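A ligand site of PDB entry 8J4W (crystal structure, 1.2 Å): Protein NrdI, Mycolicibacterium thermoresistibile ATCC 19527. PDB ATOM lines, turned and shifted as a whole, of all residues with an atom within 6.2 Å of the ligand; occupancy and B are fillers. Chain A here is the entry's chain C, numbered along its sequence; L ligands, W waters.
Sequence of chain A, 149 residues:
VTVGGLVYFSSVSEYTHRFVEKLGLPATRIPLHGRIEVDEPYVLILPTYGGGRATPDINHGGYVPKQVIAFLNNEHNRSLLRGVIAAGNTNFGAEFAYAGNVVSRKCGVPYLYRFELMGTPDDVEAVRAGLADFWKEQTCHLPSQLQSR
O of Gly 50 sits close to N3 of the ligand, 2.9 Å away.
Merely in contact with the ligand: Pro 47 (3.2 Å), Gly 88 (3.2 Å), Phe 96 (3.3 Å), Phe 92 (3.3 Å), Leu 117 (3.4 Å), Gly 51 (3.4 Å), Ala 87 (3.8 Å) and Tyr 63 (3.9 Å).
Hydrophobic or aromatic side chains within 4 Å of the ligand: Tyr 15, Pro 47, Tyr 49, Tyr 63, Phe 92, Phe 96 and Leu 117.
Of the 28 residues printed, 20 come within 4 Å of the ligand.
The side-chain hydroxyl (OG) of Ser 13 lies within hydrogen-bond range of an oxygen (O7) of the ligand (2.5 Å).
OH of Tyr 49 lies within hydrogen-bond range of O9 of the ligand.
The backbone NH (N) of Ser 11 is in hydrogen-bond range of an oxygen (O9) of the ligand.
The side-chain hydroxyl (OG) of Ser 11 sits at hydrogen-bond distance from an oxygen (O9) of the ligand (2.7 Å).
The backbone NH (N) of Thr 48 lies within hydrogen-bond range of an oxygen (O3) of the ligand (3.3 Å).
An oxygen (O3) of the ligand sits at hydrogen-bond distance from the backbone carbonyl oxygen (O) of Thr 48 (2.7 Å).
OG of Ser 10 lies within hydrogen-bond range of O8 of the ligand, 2.7 Å away.
N of Thr 16 lies within hydrogen-bond range of O8 of the ligand (2.9 Å).
O8 of the ligand lies within hydrogen-bond range of OG1 of Thr 16, at 2.7 Å.
An oxygen (O1) of the ligand lies within hydrogen-bond range of the backbone NH (N) of Ala 97, 2.8 Å away.
N of Tyr 15 sits at hydrogen-bond distance from O7 of the ligand (2.8 Å).
N2 of the ligand lies within hydrogen-bond range of O of Glu 95 (2.9 Å).
The backbone NH (N) of Asn 89 is in hydrogen-bond range of an oxygen (O1) of the ligand, 2.9 Å away.
The backbone NH of Glu 14 is in hydrogen-bond range of an oxygen (O7) of the ligand (3.2 Å).
The side-chain hydroxyl (OG) of Ser 11 lies within hydrogen-bond range of the side-chain hydroxyl (OG) of Ser 13, 3.0 Å away.
The backbone carbonyl oxygen (O) of Ala 87 lies within hydrogen-bond range of the side-chain hydroxyl (OG1) of Thr 48, at 2.9 Å.
The side-chain hydroxyl of Thr 48 is in hydrogen-bond range of the backbone NH of Tyr 98 (3.3 Å).
OG of Ser 10 lies within hydrogen-bond range of N of Thr 16, at 3.4 Å.
The backbone NH of His 17 lies within hydrogen-bond range of the side-chain hydroxyl of Ser 10.
OE1 of Glu 95 lies within hydrogen-bond range of OH of Tyr 63 (2.5 Å).
OE2 of Glu 95 sits at hydrogen-bond distance from N of Gly 52, 2.7 Å away.
N of Leu 117 is in hydrogen-bond range of O of Gly 88 (3.0 Å).
Water W1 lies within hydrogen-bond range of O5 of the ligand, O of Leu 117 and OG1 of Thr 16.
Water W2 lies within hydrogen-bond range of O4 of the ligand (2.9 Å) and OG of Ser 13 (3.0 Å).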
ATOM      1  N   PHE A   9      12.909 -11.205  -3.935  1.00  0.00           N
ATOM      2  CA  PHE A   9      12.032 -10.442  -3.036  1.00  0.00           C
ATOM      3  C   PHE A   9      10.754 -10.098  -3.790  1.00  0.00           C
ATOM      4  O   PHE A   9      10.787  -9.853  -5.000  1.00  0.00           O
ATOM      5  CB  PHE A   9      12.697  -9.151  -2.540  1.00  0.00           C
ATOM      6  CG  PHE A   9      11.821  -8.357  -1.620  1.00  0.00           C
ATOM      7  CD1 PHE A   9      11.736  -8.700  -0.289  1.00  0.00           C
ATOM      8  CD2 PHE A   9      11.027  -7.330  -2.096  1.00  0.00           C
ATOM      9  CE1 PHE A   9      10.901  -8.019   0.572  1.00  0.00           C
ATOM     10  CE2 PHE A   9      10.186  -6.642  -1.236  1.00  0.00           C
ATOM     11  CZ  PHE A   9      10.123  -6.981   0.090  1.00  0.00           C
ATOM     12  N   SER A  10       9.629 -10.106  -3.078  1.00  0.00           N
ATOM     13  CA  SER A  10       8.368  -9.677  -3.673  1.00  0.00           C
ATOM     14  C   SER A  10       7.519  -9.045  -2.575  1.00  0.00           C
ATOM     15  O   SER A  10       7.425  -9.606  -1.483  1.00  0.00           O
ATOM     16  CB  SER A  10       7.632 -10.873  -4.282  1.00  0.00           C
ATOM     17  OG  SER A  10       6.552 -10.473  -5.116  1.00  0.00           O
ATOM     18  N   SER A  11       6.915  -7.896  -2.874  1.00  0.00           N
ATOM     19  CA  SER A  11       6.042  -7.219  -1.920  1.00  0.00           C
ATOM     20  C   SER A  11       4.637  -7.823  -1.979  1.00  0.00           C
ATOM     21  O   SER A  11       4.395  -8.838  -2.636  1.00  0.00           O
ATOM     22  CB  SER A  11       5.969  -5.732  -2.224  1.00  0.00           C
ATOM     23  OG  SER A  11       5.080  -5.504  -3.319  1.00  0.00           O
ATOM     24  N   VAL A  12       3.688  -7.136  -1.332  1.00  0.00           N
ATOM     25  CA  VAL A  12       2.283  -7.550  -1.324  1.00  0.00           C
ATOM     26  C   VAL A  12       1.662  -7.671  -2.697  1.00  0.00           C
ATOM     27  O   VAL A  12       0.657  -8.378  -2.855  1.00  0.00           O
ATOM     28  CB  VAL A  12       1.416  -6.640  -0.439  1.00  0.00           C
ATOM     29  CG1 VAL A  12       1.897  -6.709   0.929  1.00  0.00           C
ATOM     30  CG2 VAL A  12       1.486  -5.202  -0.948  1.00  0.00           C
ATOM     31  N   SER A  13       2.179  -6.942  -3.682  1.00  0.00           N
ATOM     32  CA  SER A  13       1.612  -7.100  -5.015  1.00  0.00           C
ATOM     33  C   SER A  13       1.963  -8.449  -5.643  1.00  0.00           C
ATOM     34  O   SER A  13       1.269  -8.881  -6.573  1.00  0.00           O
ATOM     35  CB  SER A  13       1.980  -5.917  -5.919  1.00  0.00           C
ATOM     36  OG  SER A  13       3.331  -5.542  -5.775  1.00  0.00           O
ATOM     37  N   GLU A  14       3.002  -9.124  -5.162  1.00  0.00           N
ATOM     38  CA  GLU A  14       3.315 -10.505  -5.523  1.00  0.00           C
ATOM     39  C   GLU A  14       3.712 -10.696  -6.981  1.00  0.00           C
ATOM     40  O   GLU A  14       3.691 -11.829  -7.470  1.00  0.00           O
ATOM     41  CB  GLU A  14       2.169 -11.473  -5.195  1.00  0.00           C
ATOM     42  CG  GLU A  14       1.681 -11.488  -3.744  1.00  0.00           C
ATOM     43  CD  GLU A  14       2.737 -11.959  -2.772  1.00  0.00           C
ATOM     44  OE1 GLU A  14       3.682 -12.672  -3.181  1.00  0.00           O
ATOM     45  OE2 GLU A  14       2.574 -11.692  -1.558  1.00  0.00           O
ATOM     46  N   TYR A  15       4.086  -9.638  -7.696  1.00  0.00           N
ATOM     47  CA  TYR A  15       4.389  -9.797  -9.110  1.00  0.00           C
ATOM     48  C   TYR A  15       5.673 -10.582  -9.331  1.00  0.00           C
ATOM     49  O   TYR A  15       5.735 -11.451 -10.224  1.00  0.00           O
ATOM     50  CB  TYR A  15       4.452  -8.452  -9.831  1.00  0.00           C
ATOM     51  CG  TYR A  15       3.183  -7.639  -9.784  1.00  0.00           C
ATOM     52  CD1 TYR A  15       1.940  -8.244  -9.886  1.00  0.00           C
ATOM     53  CD2 TYR A  15       3.226  -6.259  -9.685  1.00  0.00           C
ATOM     54  CE1 TYR A  15       0.767  -7.492  -9.861  1.00  0.00           C
ATOM     55  CE2 TYR A  15       2.064  -5.486  -9.659  1.00  0.00           C
ATOM     56  CZ  TYR A  15       0.832  -6.115  -9.741  1.00  0.00           C
ATOM     57  OH  TYR A  15      -0.336  -5.374  -9.723  1.00  0.00           O
ATOM     58  N   THR A  16       6.721 -10.293  -8.554  1.00  0.00           N
ATOM     59  CA  THR A  16       7.959 -11.049  -8.683  1.00  0.00           C
ATOM     60  C   THR A  16       7.761 -12.490  -8.243  1.00  0.00           C
ATOM     61  O   THR A  16       8.290 -13.421  -8.860  1.00  0.00           O
ATOM     62  CB  THR A  16       9.093 -10.369  -7.916  1.00  0.00           C
ATOM     63  OG1 THR A  16       9.139  -8.977  -8.243  1.00  0.00           O
ATOM     64  CG2 THR A  16      10.433 -10.995  -8.239  1.00  0.00           C
ATOM     65  N   HIS A  17       6.970 -12.697  -7.185  1.00  0.00           N
ATOM     66  CA  HIS A  17       6.609 -14.037  -6.762  1.00  0.00           C
ATOM     67  C   HIS A  17       5.925 -14.803  -7.889  1.00  0.00           C
ATOM     68  O   HIS A  17       6.260 -15.958  -8.157  1.00  0.00           O
ATOM     69  CB  HIS A  17       5.712 -13.953  -5.533  1.00  0.00           C
ATOM     70  CG  HIS A  17       5.142 -15.258  -5.096  1.00  0.00           C
ATOM     71  ND1 HIS A  17       5.909 -16.266  -4.527  1.00  0.00           N
ATOM     72  CD2 HIS A  17       3.885 -15.747  -5.165  1.00  0.00           C
ATOM     73  CE1 HIS A  17       5.139 -17.291  -4.247  1.00  0.00           C
ATOM     74  NE2 HIS A  17       3.910 -17.010  -4.627  1.00  0.00           N
ATOM     75  N   PRO A  47      12.397  -6.578  -7.509  1.00  0.00           N
ATOM     76  CA  PRO A  47      11.680  -5.443  -8.090  1.00  0.00           C
ATOM     77  C   PRO A  47      12.316  -4.135  -7.640  1.00  0.00           C
ATOM     78  O   PRO A  47      13.207  -4.081  -6.795  1.00  0.00           O
ATOM     79  CB  PRO A  47      10.283  -5.613  -7.475  1.00  0.00           C
ATOM     80  CG  PRO A  47      10.579  -6.152  -6.097  1.00  0.00           C
ATOM     81  CD  PRO A  47      11.752  -7.093  -6.287  1.00  0.00           C
ATOM     82  N   THR A  48      11.818  -3.054  -8.240  1.00  0.00           N
ATOM     83  CA  THR A  48      12.325  -1.701  -8.007  1.00  0.00           C
ATOM     84  C   THR A  48      11.262  -0.849  -7.333  1.00  0.00           C
ATOM     85  O   THR A  48      10.122  -0.782  -7.794  1.00  0.00           O
ATOM     86  CB  THR A  48      12.705  -1.049  -9.345  1.00  0.00           C
ATOM     87  OG1 THR A  48      13.622  -1.905 -10.041  1.00  0.00           O
ATOM     88  CG2 THR A  48      13.333   0.304  -9.128  1.00  0.00           C
ATOM     89  N   TYR A  49      11.633  -0.181  -6.236  1.00  0.00           N
ATOM     90  CA  TYR A  49      10.720   0.767  -5.597  1.00  0.00           C
ATOM     91  C   TYR A  49      11.294   2.173  -5.684  1.00  0.00           C
ATOM     92  O   TYR A  49      12.148   2.454  -6.520  1.00  0.00           O
ATOM     93  CB  TYR A  49      10.420   0.339  -4.151  1.00  0.00           C
ATOM     94  CG  TYR A  49       9.877  -1.056  -4.061  1.00  0.00           C
ATOM     95  CD1 TYR A  49       8.901  -1.523  -4.930  1.00  0.00           C
ATOM     96  CD2 TYR A  49      10.421  -1.945  -3.142  1.00  0.00           C
ATOM     97  CE1 TYR A  49       8.440  -2.854  -4.843  1.00  0.00           C
ATOM     98  CE2 TYR A  49       9.965  -3.246  -3.056  1.00  0.00           C
ATOM     99  CZ  TYR A  49       8.985  -3.699  -3.909  1.00  0.00           C
ATOM    100  OH  TYR A  49       8.585  -5.024  -3.788  1.00  0.00           O
ATOM    101  N   GLY A  50      10.776   3.084  -4.845  1.00  0.00           N
ATOM    102  CA  GLY A  50      11.258   4.440  -4.901  1.00  0.00           C
ATOM    103  C   GLY A  50      10.924   5.078  -6.237  1.00  0.00           C
ATOM    104  O   GLY A  50       9.836   4.895  -6.802  1.00  0.00           O
ATOM    105  N   GLY A  51      11.876   5.822  -6.767  1.00  0.00           N
ATOM    106  CA  GLY A  51      11.707   6.369  -8.100  1.00  0.00           C
ATOM    107  C   GLY A  51      10.970   7.686  -8.123  1.00  0.00           C
ATOM    108  O   GLY A  51      10.706   8.327  -7.105  1.00  0.00           O
ATOM    109  N   GLY A  52      10.619   8.091  -9.356  1.00  0.00           N
ATOM    110  CA  GLY A  52      10.033   9.380  -9.625  1.00  0.00           C
ATOM    111  C   GLY A  52      10.984  10.396 -10.205  1.00  0.00           C
ATOM    112  O   GLY A  52      10.534  11.452 -10.662  1.00  0.00           O
ATOM    113  N   TYR A  63      15.604   2.621  -4.541  1.00  0.00           N
ATOM    114  CA  TYR A  63      15.286   1.708  -5.637  1.00  0.00           C
ATOM    115  C   TYR A  63      15.360   0.251  -5.183  1.00  0.00           C
ATOM    116  O   TYR A  63      14.471  -0.553  -5.502  1.00  0.00           O
ATOM    117  CB  TYR A  63      16.228   1.923  -6.815  1.00  0.00           C
ATOM    118  CG  TYR A  63      16.119   3.277  -7.441  1.00  0.00           C
ATOM    119  CD1 TYR A  63      14.989   3.642  -8.169  1.00  0.00           C
ATOM    120  CD2 TYR A  63      17.138   4.201  -7.293  1.00  0.00           C
ATOM    121  CE1 TYR A  63      14.888   4.899  -8.748  1.00  0.00           C
ATOM    122  CE2 TYR A  63      17.050   5.446  -7.859  1.00  0.00           C
ATOM    123  CZ  TYR A  63      15.932   5.792  -8.591  1.00  0.00           C
ATOM    124  OH  TYR A  63      15.845   7.041  -9.147  1.00  0.00           O
ATOM    125  N   ALA A  87      12.948  -6.324 -11.889  1.00  0.00           N
ATOM    126  CA  ALA A  87      11.622  -6.031 -12.368  1.00  0.00           C
ATOM    127  C   ALA A  87      11.272  -4.576 -12.106  1.00  0.00           C
ATOM    128  O   ALA A  87      11.814  -3.921 -11.209  1.00  0.00           O
ATOM    129  CB  ALA A  87      10.596  -6.936 -11.691  1.00  0.00           C
ATOM    130  N   GLY A  88      10.324  -4.089 -12.904  1.00  0.00           N
ATOM    131  CA  GLY A  88       9.811  -2.750 -12.738  1.00  0.00           C
ATOM    132  C   GLY A  88       8.622  -2.507 -13.637  1.00  0.00           C
ATOM    133  O   GLY A  88       7.884  -3.425 -13.997  1.00  0.00           O
ATOM    134  N   ASN A  89       8.457  -1.241 -14.006  1.00  0.00           N
ATOM    135  CA  ASN A  89       7.361  -0.730 -14.816  1.00  0.00           C
ATOM    136  C   ASN A  89       7.948   0.283 -15.780  1.00  0.00           C
ATOM    137  O   ASN A  89       8.530   1.271 -15.340  1.00  0.00           O
ATOM    138  CB  ASN A  89       6.309  -0.076 -13.906  1.00  0.00           C
ATOM    139  CG  ASN A  89       5.053   0.306 -14.634  1.00  0.00           C
ATOM    140  OD1 ASN A  89       5.113   0.773 -15.782  1.00  0.00           O
ATOM    141  ND2 ASN A  89       3.903   0.099 -14.005  1.00  0.00           N
ATOM    142  N   THR A  90       7.820   0.033 -17.092  1.00  0.00           N
ATOM    143  CA  THR A  90       8.471   0.913 -18.056  1.00  0.00           C
ATOM    144  C   THR A  90       7.902   2.328 -18.063  1.00  0.00           C
ATOM    145  O   THR A  90       8.530   3.218 -18.649  1.00  0.00           O
ATOM    146  CB  THR A  90       8.458   0.369 -19.485  1.00  0.00           C
ATOM    147  OG1 THR A  90       7.096   0.216 -19.918  1.00  0.00           O
ATOM    148  CG2 THR A  90       9.220  -0.955 -19.603  1.00  0.00           C
ATOM    149  N   PHE A  92       8.183   4.162 -15.729  1.00  0.00           N
ATOM    150  CA  PHE A  92       9.240   4.879 -15.031  1.00  0.00           C
ATOM    151  C   PHE A  92      10.393   5.297 -15.937  1.00  0.00           C
ATOM    152  O   PHE A  92      11.300   5.980 -15.454  1.00  0.00           O
ATOM    153  CB  PHE A  92       9.742   4.027 -13.862  1.00  0.00           C
ATOM    154  CG  PHE A  92       8.864   4.088 -12.626  1.00  0.00           C
ATOM    155  CD1 PHE A  92       9.090   5.052 -11.645  1.00  0.00           C
ATOM    156  CD2 PHE A  92       7.822   3.198 -12.450  1.00  0.00           C
ATOM    157  CE1 PHE A  92       8.295   5.089 -10.498  1.00  0.00           C
ATOM    158  CE2 PHE A  92       7.020   3.239 -11.314  1.00  0.00           C
ATOM    159  CZ  PHE A  92       7.257   4.184 -10.338  1.00  0.00           C
ATOM    160  N   GLU A  95      14.083   5.235 -15.055  1.00  0.00           N
ATOM    161  CA  GLU A  95      14.163   4.489 -13.807  1.00  0.00           C
ATOM    162  C   GLU A  95      13.643   3.065 -13.935  1.00  0.00           C
ATOM    163  O   GLU A  95      13.480   2.377 -12.914  1.00  0.00           O
ATOM    164  CB  GLU A  95      13.392   5.200 -12.695  1.00  0.00           C
ATOM    165  CG  GLU A  95      14.064   6.436 -12.180  1.00  0.00           C
ATOM    166  CD  GLU A  95      13.157   7.229 -11.276  1.00  0.00           C
ATOM    167  OE1 GLU A  95      13.613   7.645 -10.201  1.00  0.00           O
ATOM    168  OE2 GLU A  95      11.964   7.404 -11.620  1.00  0.00           O
ATOM    169  N   PHE A  96      13.323   2.614 -15.144  1.00  0.00           N
ATOM    170  CA  PHE A  96      12.770   1.267 -15.320  1.00  0.00           C
ATOM    171  C   PHE A  96      13.712   0.205 -14.785  1.00  0.00           C
ATOM    172  O   PHE A  96      14.857   0.096 -15.227  1.00  0.00           O
ATOM    173  CB  PHE A  96      12.508   0.972 -16.791  1.00  0.00           C
ATOM    174  CG  PHE A  96      12.136  -0.466 -17.052  1.00  0.00           C
ATOM    175  CD1 PHE A  96      11.104  -1.068 -16.351  1.00  0.00           C
ATOM    176  CD2 PHE A  96      12.861  -1.231 -17.953  1.00  0.00           C
ATOM    177  CE1 PHE A  96      10.760  -2.393 -16.573  1.00  0.00           C
ATOM    178  CE2 PHE A  96      12.537  -2.566 -18.174  1.00  0.00           C
ATOM    179  CZ  PHE A  96      11.495  -3.140 -17.482  1.00  0.00           C
ATOM    180  N   ALA A  97      13.204  -0.591 -13.829  1.00  0.00           N
ATOM    181  CA  ALA A  97      13.949  -1.725 -13.273  1.00  0.00           C
ATOM    182  C   ALA A  97      15.295  -1.287 -12.711  1.00  0.00           C
ATOM    183  O   ALA A  97      16.252  -2.056 -12.701  1.00  0.00           O
ATOM    184  CB  ALA A  97      14.090  -2.842 -14.297  1.00  0.00           C
ATOM    185  N   TYR A  98      15.362  -0.060 -12.199  1.00  0.00           N
ATOM    186  CA  TYR A  98      16.638   0.548 -11.812  1.00  0.00           C
ATOM    187  C   TYR A  98      17.323  -0.193 -10.666  1.00  0.00           C
ATOM    188  O   TYR A  98      18.534  -0.023 -10.490  1.00  0.00           O
ATOM    189  CB  TYR A  98      16.427   2.006 -11.418  1.00  0.00           C
ATOM    190  CG  TYR A  98      17.590   2.916 -11.672  1.00  0.00           C
ATOM    191  CD1 TYR A  98      18.076   3.107 -12.953  1.00  0.00           C
ATOM    192  CD2 TYR A  98      18.117   3.687 -10.645  1.00  0.00           C
ATOM    193  CE1 TYR A  98      19.110   3.981 -13.209  1.00  0.00           C
ATOM    194  CE2 TYR A  98      19.140   4.580 -10.896  1.00  0.00           C
ATOM    195  CZ  TYR A  98      19.639   4.715 -12.179  1.00  0.00           C
ATOM    196  OH  TYR A  98      20.656   5.606 -12.417  1.00  0.00           O
ATOM    197  N   GLU A 116       8.886  -6.548 -16.811  1.00  0.00           N
ATOM    198  CA  GLU A 116       7.825  -5.724 -16.245  1.00  0.00           C
ATOM    199  C   GLU A 116       6.870  -6.592 -15.451  1.00  0.00           C
ATOM    200  O   GLU A 116       6.388  -7.609 -15.947  1.00  0.00           O
ATOM    201  CB  GLU A 116       7.032  -5.080 -17.383  1.00  0.00           C
ATOM    202  CG  GLU A 116       7.625  -3.845 -17.947  1.00  0.00           C
ATOM    203  CD  GLU A 116       6.557  -3.068 -18.679  1.00  0.00           C
ATOM    204  OE1 GLU A 116       6.086  -3.579 -19.727  1.00  0.00           O
ATOM    205  OE2 GLU A 116       6.159  -1.982 -18.204  1.00  0.00           O
ATOM    206  N   LEU A 117       6.557  -6.155 -14.229  1.00  0.00           N
ATOM    207  CA  LEU A 117       5.498  -6.758 -13.406  1.00  0.00           C
ATOM    208  C   LEU A 117       5.736  -8.259 -13.290  1.00  0.00           C
ATOM    209  O   LEU A 117       6.832  -8.684 -12.913  1.00  0.00           O
ATOM    210  CB  LEU A 117       4.107  -6.342 -13.870  1.00  0.00           C
ATOM    211  CG  LEU A 117       3.866  -4.852 -14.111  1.00  0.00           C
ATOM    212  CD1 LEU A 117       2.472  -4.586 -14.679  1.00  0.00           C
ATOM    213  CD2 LEU A 117       4.104  -4.107 -12.831  1.00  0.00           C
ATOM    214  N   MET A 118       4.735  -9.095 -13.593  1.00  0.00           N
ATOM    215  CA  MET A 118       4.871 -10.528 -13.458  1.00  0.00           C
ATOM    216  C   MET A 118       5.535 -11.201 -14.646  1.00  0.00           C
ATOM    217  O   MET A 118       5.661 -12.428 -14.632  1.00  0.00           O
ATOM    218  CB  MET A 118       3.538 -11.233 -13.153  1.00  0.00           C
ATOM    219  CG  MET A 118       2.361 -11.062 -14.112  1.00  0.00           C
ATOM    220  SD  MET A 118       1.862  -9.429 -14.698  1.00  0.00           S
ATOM    221  CE  MET A 118       0.970  -8.841 -13.265  1.00  0.00           C
HETATM  222  N1  LIG L   1       9.284   0.338 -11.236  1.00  0.00           N
HETATM  223  C1  LIG L   1      10.390   0.805 -11.884  1.00  0.00           C
HETATM  224  O1  LIG L   1      10.712   0.321 -12.970  1.00  0.00           O
HETATM  225  N2  LIG L   1      11.114   1.827 -11.347  1.00  0.00           N
HETATM  226  C2  LIG L   1      10.760   2.419 -10.157  1.00  0.00           C
HETATM  227  O2  LIG L   1      11.475   3.350  -9.735  1.00  0.00           O
HETATM  228  C3  LIG L   1       9.633   1.943  -9.481  1.00  0.00           C
HETATM  229  N3  LIG L   1       9.222   2.493  -8.280  1.00  0.00           N
HETATM  230  C4  LIG L   1       8.097   2.005  -7.653  1.00  0.00           C
HETATM  231  C5  LIG L   1       7.681   2.566  -6.444  1.00  0.00           C
HETATM  232  C6  LIG L   1       6.558   2.075  -5.785  1.00  0.00           C
HETATM  233  C7  LIG L   1       6.136   2.686  -4.475  1.00  0.00           C
HETATM  234  C8  LIG L   1       5.829   1.029  -6.345  1.00  0.00           C
HETATM  235  C9  LIG L   1       4.604   0.488  -5.674  1.00  0.00           C
HETATM  236  C10 LIG L   1       6.238   0.475  -7.555  1.00  0.00           C
HETATM  237  C11 LIG L   1       7.367   0.955  -8.222  1.00  0.00           C
HETATM  238  N4  LIG L   1       7.783   0.397  -9.422  1.00  0.00           N
HETATM  239  C12 LIG L   1       8.904   0.896 -10.041  1.00  0.00           C
HETATM  240  C13 LIG L   1       7.052  -0.764 -10.056  1.00  0.00           C
HETATM  241  C14 LIG L   1       7.403  -2.083  -9.334  1.00  0.00           C
HETATM  242  O3  LIG L   1       8.774  -2.397  -9.425  1.00  0.00           O
HETATM  243  C15 LIG L   1       6.592  -3.204  -9.973  1.00  0.00           C
HETATM  244  O4  LIG L   1       5.212  -3.007  -9.718  1.00  0.00           O
HETATM  245  C16 LIG L   1       7.042  -4.598  -9.517  1.00  0.00           C
HETATM  246  O5  LIG L   1       6.449  -5.530 -10.375  1.00  0.00           O
HETATM  247  C17 LIG L   1       6.625  -4.912  -8.078  1.00  0.00           C
HETATM  248  O6  LIG L   1       7.143  -6.197  -7.747  1.00  0.00           O
HETATM  249  P1  LIG L   1       6.507  -6.973  -6.502  1.00  0.00           P
HETATM  250  O7  LIG L   1       5.020  -7.131  -6.743  1.00  0.00           O
HETATM  251  O8  LIG L   1       7.191  -8.290  -6.515  1.00  0.00           O
HETATM  252  O9  LIG L   1       6.770  -6.190  -5.251  1.00  0.00           O
HETATM  253  O   HOH W   1       7.775  -7.869 -10.489  1.00  0.00           O
HETATM  254  O   HOH W   2       3.985  -2.990  -7.114  1.00  0.00           O
